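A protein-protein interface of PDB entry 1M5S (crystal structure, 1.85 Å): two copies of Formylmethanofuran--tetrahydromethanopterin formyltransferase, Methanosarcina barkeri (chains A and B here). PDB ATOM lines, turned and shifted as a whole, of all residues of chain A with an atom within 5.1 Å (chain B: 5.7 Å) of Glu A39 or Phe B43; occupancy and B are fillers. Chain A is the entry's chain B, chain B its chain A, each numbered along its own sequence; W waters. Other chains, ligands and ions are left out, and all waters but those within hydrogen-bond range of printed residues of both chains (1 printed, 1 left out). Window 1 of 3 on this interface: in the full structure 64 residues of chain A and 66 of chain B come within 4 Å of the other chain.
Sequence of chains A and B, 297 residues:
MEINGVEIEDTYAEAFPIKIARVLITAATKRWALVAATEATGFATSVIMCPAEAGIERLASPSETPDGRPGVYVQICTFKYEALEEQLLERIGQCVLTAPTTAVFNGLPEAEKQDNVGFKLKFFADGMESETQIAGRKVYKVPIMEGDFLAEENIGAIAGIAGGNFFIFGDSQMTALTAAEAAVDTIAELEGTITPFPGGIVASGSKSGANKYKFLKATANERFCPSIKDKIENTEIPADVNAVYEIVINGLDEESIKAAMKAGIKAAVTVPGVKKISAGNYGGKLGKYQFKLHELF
Among the printed residues, pairs that only touch across the chains: Cys A95 with Pro B198 (3.3 Å), Glu A90 with Phe B43 (3.4 Å), Phe A43 with Arg B91 (3.4 Å), Glu A39 with Thr B45 (3.4 Å), Val A35 with Gly B199 (3.4 Å), Gly A42 with Phe B43 (3.6 Å), Phe A43 with Gly B42 (3.7 Å), Glu A39 with Gly B42 (3.7 Å), Gln A87 with Phe B43 (3.7 Å), Arg A91 with Phe B43 (3.8 Å), Cys A95 with Phe B43 (3.8 Å), Val A35 with Pro B198 (3.8 Å), Glu A90 with Met B49 (3.8 Å) and Glu A39 with Thr B41 (3.9 Å).
The backbone carbonyl oxygen of Phe B43 is in hydrogen-bond range of the guanidinium group of Arg B91 (3.0 Å). NH1 of Arg B91 lies within hydrogen-bond range of O of Gly B42, 2.8 Å away. NH1 of Arg A91 is in hydrogen-bond range of O of Gly A42. NE2 of Gln A87 lies close to NE of Arg A91 (2.8 Å). The backbone carbonyl oxygen (O) of Phe A43 is in hydrogen-bond range of the guanidinium group (NH2) of Arg A91 (3.1 Å). N of Thr B45 lies within hydrogen-bond range of SG of Cys B50, at 3.6 Å.
Gly A42 touches Phe B43, and with the chains exchanged Phe A43 touches Gly B42. Phe A43 touches Arg B91, and with the chains exchanged Arg A91 touches Phe B43. Of the 16 pairs that touch across the chains among the printed residues, 4 have their exchanged pair printed and touching as well.
Hydrophobic or aromatic side chains of chain A within 4 Å of the printed part of chain B: Val A35 and Phe A43. Hydrophobic or aromatic side chains of chain B within 4 Å of the printed part of chain A: Phe B43 and Pro B198. Among the printed residues, 16 pairs touch across the chains. Among the printed residues, no Asp or Glu carboxylate lies within 4 Å of a Lys or Arg side-chain nitrogen of the other chain.
Glu A39 touches five residues of chain B. Of chain A, only Glu A39 (3.0 Å), Gly A42 (3.6 Å), Gln A87 (3.7 Å), Glu A90 (3.4 Å), Arg A91 (3.8 Å) and Cys A95 (3.8 Å) come within 4 Å of Phe B43. Printed residues of chain B within 4 Å of Arg A91: Phe B43. Of the printed residues of chain A, Thr B45 touches Glu A39. The nearest printed residue of chain B that does not touch Val A35 is Phe B197 (6.4 Å).
The side-chain carboxylate of Glu A39 is in hydrogen-bond range of the backbone NH of Ala B44, at 3.3 Å. N of Phe B43 sits at hydrogen-bond distance from O of Glu A39.
Water W1 lies within hydrogen-bond range of the backbone NH (N) of Gly B199 (2.9 Å), the side-chain carboxylate (OE1) of Glu A39 (2.9 Å) and the backbone carbonyl oxygen (O) of Phe B197 (3.5 Å).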
ATOM      1  N   LEU A  34      19.497 -18.167  10.192  1.00  0.00           N
ATOM      2  CA  LEU A  34      19.913 -17.158   9.222  1.00  0.00           C
ATOM      3  C   LEU A  34      18.710 -16.538   8.509  1.00  0.00           C
ATOM      4  O   LEU A  34      18.735 -15.361   8.150  1.00  0.00           O
ATOM      5  CB  LEU A  34      20.876 -17.760   8.190  1.00  0.00           C
ATOM      6  CG  LEU A  34      21.382 -16.771   7.128  1.00  0.00           C
ATOM      7  CD1 LEU A  34      22.179 -15.669   7.808  1.00  0.00           C
ATOM      8  CD2 LEU A  34      22.245 -17.475   6.087  1.00  0.00           C
ATOM      9  N   VAL A  35      17.673 -17.345   8.281  1.00  0.00           N
ATOM     10  CA  VAL A  35      16.441 -16.885   7.650  1.00  0.00           C
ATOM     11  C   VAL A  35      15.783 -15.801   8.512  1.00  0.00           C
ATOM     12  O   VAL A  35      15.477 -14.708   8.027  1.00  0.00           O
ATOM     13  CB  VAL A  35      15.464 -18.069   7.458  1.00  0.00           C
ATOM     14  CG1 VAL A  35      14.056 -17.577   7.222  1.00  0.00           C
ATOM     15  CG2 VAL A  35      15.912 -18.912   6.299  1.00  0.00           C
ATOM     16  N   ALA A  36      15.676 -16.071   9.812  1.00  0.00           N
ATOM     17  CA  ALA A  36      15.069 -15.130  10.749  1.00  0.00           C
ATOM     18  C   ALA A  36      15.921 -13.874  10.904  1.00  0.00           C
ATOM     19  O   ALA A  36      15.408 -12.765  10.808  1.00  0.00           O
ATOM     20  CB  ALA A  36      14.867 -15.795  12.098  1.00  0.00           C
ATOM     21  N   ALA A  37      17.231 -14.059  11.068  1.00  0.00           N
ATOM     22  CA  ALA A  37      18.176 -12.945  11.232  1.00  0.00           C
ATOM     23  C   ALA A  37      18.218 -12.012  10.022  1.00  0.00           C
ATOM     24  O   ALA A  37      18.335 -10.792  10.172  1.00  0.00           O
ATOM     25  CB  ALA A  37      19.568 -13.487  11.516  1.00  0.00           C
ATOM     26  N   THR A  38      18.127 -12.594   8.828  1.00  0.00           N
ATOM     27  CA  THR A  38      18.099 -11.831   7.586  1.00  0.00           C
ATOM     28  C   THR A  38      16.830 -10.997   7.491  1.00  0.00           C
ATOM     29  O   THR A  38      16.893  -9.796   7.215  1.00  0.00           O
ATOM     30  CB  THR A  38      18.181 -12.767   6.371  1.00  0.00           C
ATOM     31  OG1 THR A  38      19.421 -13.482   6.418  1.00  0.00           O
ATOM     32  CG2 THR A  38      18.116 -11.987   5.076  1.00  0.00           C
ATOM     33  N   GLU A  39      15.687 -11.643   7.723  1.00  0.00           N
ATOM     34  CA  GLU A  39      14.388 -10.976   7.695  1.00  0.00           C
ATOM     35  C   GLU A  39      14.304  -9.836   8.725  1.00  0.00           C
ATOM     36  O   GLU A  39      13.857  -8.723   8.410  1.00  0.00           O
ATOM     37  CB  GLU A  39      13.276 -11.998   7.952  1.00  0.00           C
ATOM     38  CG  GLU A  39      11.856 -11.415   7.913  1.00  0.00           C
ATOM     39  CD  GLU A  39      11.418 -10.964   6.527  1.00  0.00           C
ATOM     40  OE1 GLU A  39      11.876 -11.557   5.529  1.00  0.00           O
ATOM     41  OE2 GLU A  39      10.566 -10.052   6.435  1.00  0.00           O
ATOM     42  N   ALA A  40      14.774 -10.115   9.937  1.00  0.00           N
ATOM     43  CA  ALA A  40      14.771  -9.151  11.031  1.00  0.00           C
ATOM     44  C   ALA A  40      15.624  -7.924  10.733  1.00  0.00           C
ATOM     45  O   ALA A  40      15.322  -6.832  11.213  1.00  0.00           O
ATOM     46  CB  ALA A  40      15.262  -9.819  12.308  1.00  0.00           C
ATOM     47  N   THR A  41      16.699  -8.115   9.970  1.00  0.00           N
ATOM     48  CA  THR A  41      17.655  -7.042   9.701  1.00  0.00           C
ATOM     49  C   THR A  41      17.547  -6.468   8.283  1.00  0.00           C
ATOM     50  O   THR A  41      18.382  -5.663   7.876  1.00  0.00           O
ATOM     51  CB  THR A  41      19.108  -7.515   9.923  1.00  0.00           C
ATOM     52  OG1 THR A  41      19.387  -8.618   9.053  1.00  0.00           O
ATOM     53  CG2 THR A  41      19.326  -7.941  11.365  1.00  0.00           C
ATOM     54  N   GLY A  42      16.524  -6.882   7.539  1.00  0.00           N
ATOM     55  CA  GLY A  42      16.290  -6.329   6.213  1.00  0.00           C
ATOM     56  C   GLY A  42      15.720  -4.921   6.279  1.00  0.00           C
ATOM     57  O   GLY A  42      15.359  -4.450   7.364  1.00  0.00           O
ATOM     58  N   PHE A  43      15.675  -4.237   5.135  1.00  0.00           N
ATOM     59  CA  PHE A  43      15.224  -2.844   5.059  1.00  0.00           C
ATOM     60  C   PHE A  43      15.878  -2.010   6.169  1.00  0.00           C
ATOM     61  O   PHE A  43      15.191  -1.408   7.004  1.00  0.00           O
ATOM     62  CB  PHE A  43      13.694  -2.787   5.169  1.00  0.00           C
ATOM     63  CG  PHE A  43      13.096  -1.432   4.857  1.00  0.00           C
ATOM     64  CD1 PHE A  43      13.765  -0.515   4.044  1.00  0.00           C
ATOM     65  CD2 PHE A  43      11.819  -1.108   5.322  1.00  0.00           C
ATOM     66  CE1 PHE A  43      13.167   0.697   3.695  1.00  0.00           C
ATOM     67  CE2 PHE A  43      11.211   0.097   4.978  1.00  0.00           C
ATOM     68  CZ  PHE A  43      11.884   1.001   4.163  1.00  0.00           C
ATOM     69  N   PRO A  51      14.059   2.609   8.592  1.00  0.00           N
ATOM     70  CA  PRO A  51      13.628   2.532   9.994  1.00  0.00           C
ATOM     71  C   PRO A  51      14.791   2.281  10.950  1.00  0.00           C
ATOM     72  O   PRO A  51      14.738   2.672  12.112  1.00  0.00           O
ATOM     73  CB  PRO A  51      12.632   1.368  10.001  1.00  0.00           C
ATOM     74  CG  PRO A  51      12.179   1.245   8.570  1.00  0.00           C
ATOM     75  CD  PRO A  51      13.396   1.587   7.763  1.00  0.00           C
ATOM     76  N   GLN A  87      12.076  -0.405  17.264  1.00  0.00           N
ATOM     77  CA  GLN A  87      12.600  -1.276  16.215  1.00  0.00           C
ATOM     78  C   GLN A  87      12.773  -2.718  16.696  1.00  0.00           C
ATOM     79  O   GLN A  87      12.357  -3.659  16.011  1.00  0.00           O
ATOM     80  CB  GLN A  87      13.928  -0.737  15.679  1.00  0.00           C
ATOM     81  CG  GLN A  87      13.778   0.442  14.737  1.00  0.00           C
ATOM     82  CD  GLN A  87      12.796   0.177  13.613  1.00  0.00           C
ATOM     83  OE1 GLN A  87      11.672   0.669  13.631  1.00  0.00           O
ATOM     84  NE2 GLN A  87      13.232  -0.573  12.610  1.00  0.00           N
ATOM     85  N   GLU A  90       9.178  -4.156  16.744  1.00  0.00           N
ATOM     86  CA  GLU A  90       8.585  -4.389  15.425  1.00  0.00           C
ATOM     87  C   GLU A  90       9.344  -5.491  14.663  1.00  0.00           C
ATOM     88  O   GLU A  90       8.753  -6.311  13.964  1.00  0.00           O
ATOM     89  CB  GLU A  90       8.600  -3.093  14.595  1.00  0.00           C
ATOM     90  CG  GLU A  90       7.793  -1.936  15.184  1.00  0.00           C
ATOM     91  CD  GLU A  90       7.635  -0.771  14.228  1.00  0.00           C
ATOM     92  OE1 GLU A  90       8.018  -0.900  13.043  1.00  0.00           O
ATOM     93  OE2 GLU A  90       7.098   0.271  14.659  1.00  0.00           O
ATOM     94  N   ARG A  91      10.656  -5.508  14.816  1.00  0.00           N
ATOM     95  CA  ARG A  91      11.517  -6.442  14.068  1.00  0.00           C
ATOM     96  C   ARG A  91      11.516  -7.852  14.686  1.00  0.00           C
ATOM     97  O   ARG A  91      11.363  -8.860  13.981  1.00  0.00           O
ATOM     98  CB  ARG A  91      12.951  -5.913  14.029  1.00  0.00           C
ATOM     99  CG  ARG A  91      13.190  -4.946  12.863  1.00  0.00           C
ATOM    100  CD  ARG A  91      14.519  -4.194  12.963  1.00  0.00           C
ATOM    101  NE  ARG A  91      14.550  -2.968  12.148  1.00  0.00           N
ATOM    102  CZ  ARG A  91      14.859  -2.941  10.842  1.00  0.00           C
ATOM    103  NH1 ARG A  91      15.167  -4.065  10.181  1.00  0.00           N
ATOM    104  NH2 ARG A  91      14.889  -1.823  10.101  1.00  0.00           N
ATOM    105  N   CYS A  95       9.257 -10.547  12.822  1.00  0.00           N
ATOM    106  CA  CYS A  95      10.190 -11.209  11.922  1.00  0.00           C
ATOM    107  C   CYS A  95      10.891 -12.385  12.573  1.00  0.00           C
ATOM    108  O   CYS A  95      11.472 -13.225  11.880  1.00  0.00           O
ATOM    109  CB  CYS A  95      11.227 -10.207  11.409  1.00  0.00           C
ATOM    110  SG  CYS A  95      10.536  -8.933  10.335  1.00  0.00           S
ATOM    111  N   THR B  41      12.977  -6.650   0.588  1.00  0.00           N
ATOM    112  CA  THR B  41      11.692  -7.219   0.993  1.00  0.00           C
ATOM    113  C   THR B  41      11.717  -7.760   2.417  1.00  0.00           C
ATOM    114  O   THR B  41      10.777  -8.421   2.851  1.00  0.00           O
ATOM    115  CB  THR B  41      11.250  -8.354   0.050  1.00  0.00           C
ATOM    116  OG1 THR B  41      12.272  -9.357  -0.001  1.00  0.00           O
ATOM    117  CG2 THR B  41      10.984  -7.819  -1.354  1.00  0.00           C
ATOM    118  N   GLY B  42      12.791  -7.459   3.146  1.00  0.00           N
ATOM    119  CA  GLY B  42      12.864  -7.804   4.556  1.00  0.00           C
ATOM    120  C   GLY B  42      12.075  -6.827   5.405  1.00  0.00           C
ATOM    121  O   GLY B  42      11.612  -5.801   4.908  1.00  0.00           O
ATOM    122  N   PHE B  43      11.943  -7.135   6.696  1.00  0.00           N
ATOM    123  CA  PHE B  43      11.111  -6.353   7.614  1.00  0.00           C
ATOM    124  C   PHE B  43       9.744  -6.028   6.994  1.00  0.00           C
ATOM    125  O   PHE B  43       9.298  -4.881   6.992  1.00  0.00           O
ATOM    126  CB  PHE B  43      11.851  -5.067   8.019  1.00  0.00           C
ATOM    127  CG  PHE B  43      11.204  -4.318   9.163  1.00  0.00           C
ATOM    128  CD1 PHE B  43      10.452  -4.994  10.118  1.00  0.00           C
ATOM    129  CD2 PHE B  43      11.372  -2.943   9.293  1.00  0.00           C
ATOM    130  CE1 PHE B  43       9.876  -4.312  11.189  1.00  0.00           C
ATOM    131  CE2 PHE B  43      10.799  -2.251  10.365  1.00  0.00           C
ATOM    132  CZ  PHE B  43      10.049  -2.942  11.313  1.00  0.00           C
ATOM    133  N   ALA B  44       9.099  -7.049   6.437  1.00  0.00           N
ATOM    134  CA  ALA B  44       7.815  -6.872   5.739  1.00  0.00           C
ATOM    135  C   ALA B  44       7.044  -8.194   5.657  1.00  0.00           C
ATOM    136  O   ALA B  44       6.794  -8.724   4.565  1.00  0.00           O
ATOM    137  CB  ALA B  44       8.064  -6.377   4.311  1.00  0.00           C
ATOM    138  N   THR B  45       6.676  -8.719   6.825  1.00  0.00           N
ATOM    139  CA  THR B  45       5.898  -9.955   6.920  1.00  0.00           C
ATOM    140  C   THR B  45       4.386  -9.698   6.955  1.00  0.00           C
ATOM    141  O   THR B  45       3.610 -10.495   6.421  1.00  0.00           O
ATOM    142  CB  THR B  45       6.311 -10.807   8.166  1.00  0.00           C
ATOM    143  OG1 THR B  45       6.041 -10.082   9.372  1.00  0.00           O
ATOM    144  CG2 THR B  45       7.796 -11.160   8.116  1.00  0.00           C
ATOM    145  N   MET B  49       1.795  -4.375  11.208  1.00  0.00           N
ATOM    146  CA  MET B  49       2.837  -3.904  12.132  1.00  0.00           C
ATOM    147  C   MET B  49       4.237  -3.744  11.501  1.00  0.00           C
ATOM    148  O   MET B  49       5.200  -3.356  12.178  1.00  0.00           O
ATOM    149  CB  MET B  49       2.939  -4.838  13.336  1.00  0.00           C
ATOM    150  CG  MET B  49       2.362  -4.283  14.620  1.00  0.00           C
ATOM    151  SD  MET B  49       3.128  -5.021  16.064  1.00  0.00           S
ATOM    152  CE  MET B  49       4.276  -3.681  16.553  1.00  0.00           C
ATOM    153  N   CYS B  50       4.360  -4.147  10.236  1.00  0.00           N
ATOM    154  CA  CYS B  50       5.561  -3.912   9.439  1.00  0.00           C
ATOM    155  C   CYS B  50       5.275  -2.788   8.446  1.00  0.00           C
ATOM    156  O   CYS B  50       4.111  -2.561   8.088  1.00  0.00           O
ATOM    157  CB  CYS B  50       5.953  -5.179   8.668  1.00  0.00           C
ATOM    158  SG  CYS B  50       6.730  -6.488   9.661  1.00  0.00           S
ATOM    159  N   PRO B  51       6.327  -2.079   7.993  1.00  0.00           N
ATOM    160  CA  PRO B  51       6.162  -1.027   6.971  1.00  0.00           C
ATOM    161  C   PRO B  51       5.427  -1.499   5.709  1.00  0.00           C
ATOM    162  O   PRO B  51       4.732  -0.715   5.055  1.00  0.00           O
ATOM    163  CB  PRO B  51       7.596  -0.586   6.669  1.00  0.00           C
ATOM    164  CG  PRO B  51       8.340  -0.858   7.949  1.00  0.00           C
ATOM    165  CD  PRO B  51       7.707  -2.110   8.523  1.00  0.00           C
ATOM    166  N   ALA B  52       5.591  -2.770   5.353  1.00  0.00           N
ATOM    167  CA  ALA B  52       4.905  -3.335   4.194  1.00  0.00           C
ATOM    168  C   ALA B  52       4.790  -4.849   4.301  1.00  0.00           C
ATOM    169  O   ALA B  52       5.187  -5.449   5.305  1.00  0.00           O
ATOM    170  CB  ALA B  52       5.640  -2.961   2.907  1.00  0.00           C
ATOM    171  N   ALA B  54       5.998  -7.854   1.850  1.00  0.00           N
ATOM    172  CA  ALA B  54       6.848  -7.993   0.681  1.00  0.00           C
ATOM    173  C   ALA B  54       7.512  -9.363   0.614  1.00  0.00           C
ATOM    174  O   ALA B  54       7.629 -10.073   1.615  1.00  0.00           O
ATOM    175  CB  ALA B  54       7.902  -6.890   0.679  1.00  0.00           C
ATOM    176  N   ARG B  91      12.426   1.487  -0.200  1.00  0.00           N
ATOM    177  CA  ARG B  91      12.963   0.114  -0.308  1.00  0.00           C
ATOM    178  C   ARG B  91      13.869  -0.060  -1.541  1.00  0.00           C
ATOM    179  O   ARG B  91      14.866  -0.795  -1.504  1.00  0.00           O
ATOM    180  CB  ARG B  91      11.820  -0.896  -0.379  1.00  0.00           C
ATOM    181  CG  ARG B  91      11.407  -1.418   1.002  1.00  0.00           C
ATOM    182  CD  ARG B  91      10.020  -2.062   1.005  1.00  0.00           C
ATOM    183  NE  ARG B  91       9.463  -2.239   2.356  1.00  0.00           N
ATOM    184  CZ  ARG B  91       9.882  -3.170   3.224  1.00  0.00           C
ATOM    185  NH1 ARG B  91      10.869  -4.018   2.905  1.00  0.00           N
ATOM    186  NH2 ARG B  91       9.369  -3.336   4.451  1.00  0.00           N
ATOM    187  N   PRO B 196       5.074 -13.814   2.323  1.00  0.00           N
ATOM    188  CA  PRO B 196       5.833 -12.711   2.926  1.00  0.00           C
ATOM    189  C   PRO B 196       6.474 -12.997   4.288  1.00  0.00           C
ATOM    190  O   PRO B 196       7.290 -12.208   4.773  1.00  0.00           O
ATOM    191  CB  PRO B 196       4.800 -11.581   3.012  1.00  0.00           C
ATOM    192  CG  PRO B 196       3.494 -12.293   3.090  1.00  0.00           C
ATOM    193  CD  PRO B 196       3.656 -13.450   2.149  1.00  0.00           C
ATOM    194  N   PHE B 197       6.079 -14.085   4.942  1.00  0.00           N
ATOM    195  CA  PHE B 197       6.584 -14.357   6.285  1.00  0.00           C
ATOM    196  C   PHE B 197       8.023 -14.881   6.259  1.00  0.00           C
ATOM    197  O   PHE B 197       8.583 -15.066   5.182  1.00  0.00           O
ATOM    198  CB  PHE B 197       5.641 -15.322   7.007  1.00  0.00           C
ATOM    199  CG  PHE B 197       4.650 -14.626   7.901  1.00  0.00           C
ATOM    200  CD1 PHE B 197       3.612 -13.872   7.355  1.00  0.00           C
ATOM    201  CD2 PHE B 197       4.817 -14.632   9.283  1.00  0.00           C
ATOM    202  CE1 PHE B 197       2.765 -13.128   8.173  1.00  0.00           C
ATOM    203  CE2 PHE B 197       3.976 -13.891  10.108  1.00  0.00           C
ATOM    204  CZ  PHE B 197       2.949 -13.136   9.552  1.00  0.00           C
ATOM    205  N   PRO B 198       8.693 -14.958   7.427  1.00  0.00           N
ATOM    206  CA  PRO B 198      10.116 -15.338   7.430  1.00  0.00           C
ATOM    207  C   PRO B 198      10.366 -16.717   6.828  1.00  0.00           C
ATOM    208  O   PRO B 198       9.916 -17.731   7.363  1.00  0.00           O
ATOM    209  CB  PRO B 198      10.491 -15.293   8.907  1.00  0.00           C
ATOM    210  CG  PRO B 198       9.507 -14.318   9.504  1.00  0.00           C
ATOM    211  CD  PRO B 198       8.231 -14.622   8.786  1.00  0.00           C
ATOM    212  N   GLY B 199      11.090 -16.740   5.711  1.00  0.00           N
ATOM    213  CA  GLY B 199      11.273 -17.973   4.961  1.00  0.00           C
ATOM    214  C   GLY B 199       9.997 -18.412   4.268  1.00  0.00           C
ATOM    215  O   GLY B 199       9.898 -19.547   3.800  1.00  0.00           O
HETATM  216  O   HOH W   1      11.900 -14.263   4.473  1.00  0.00           O
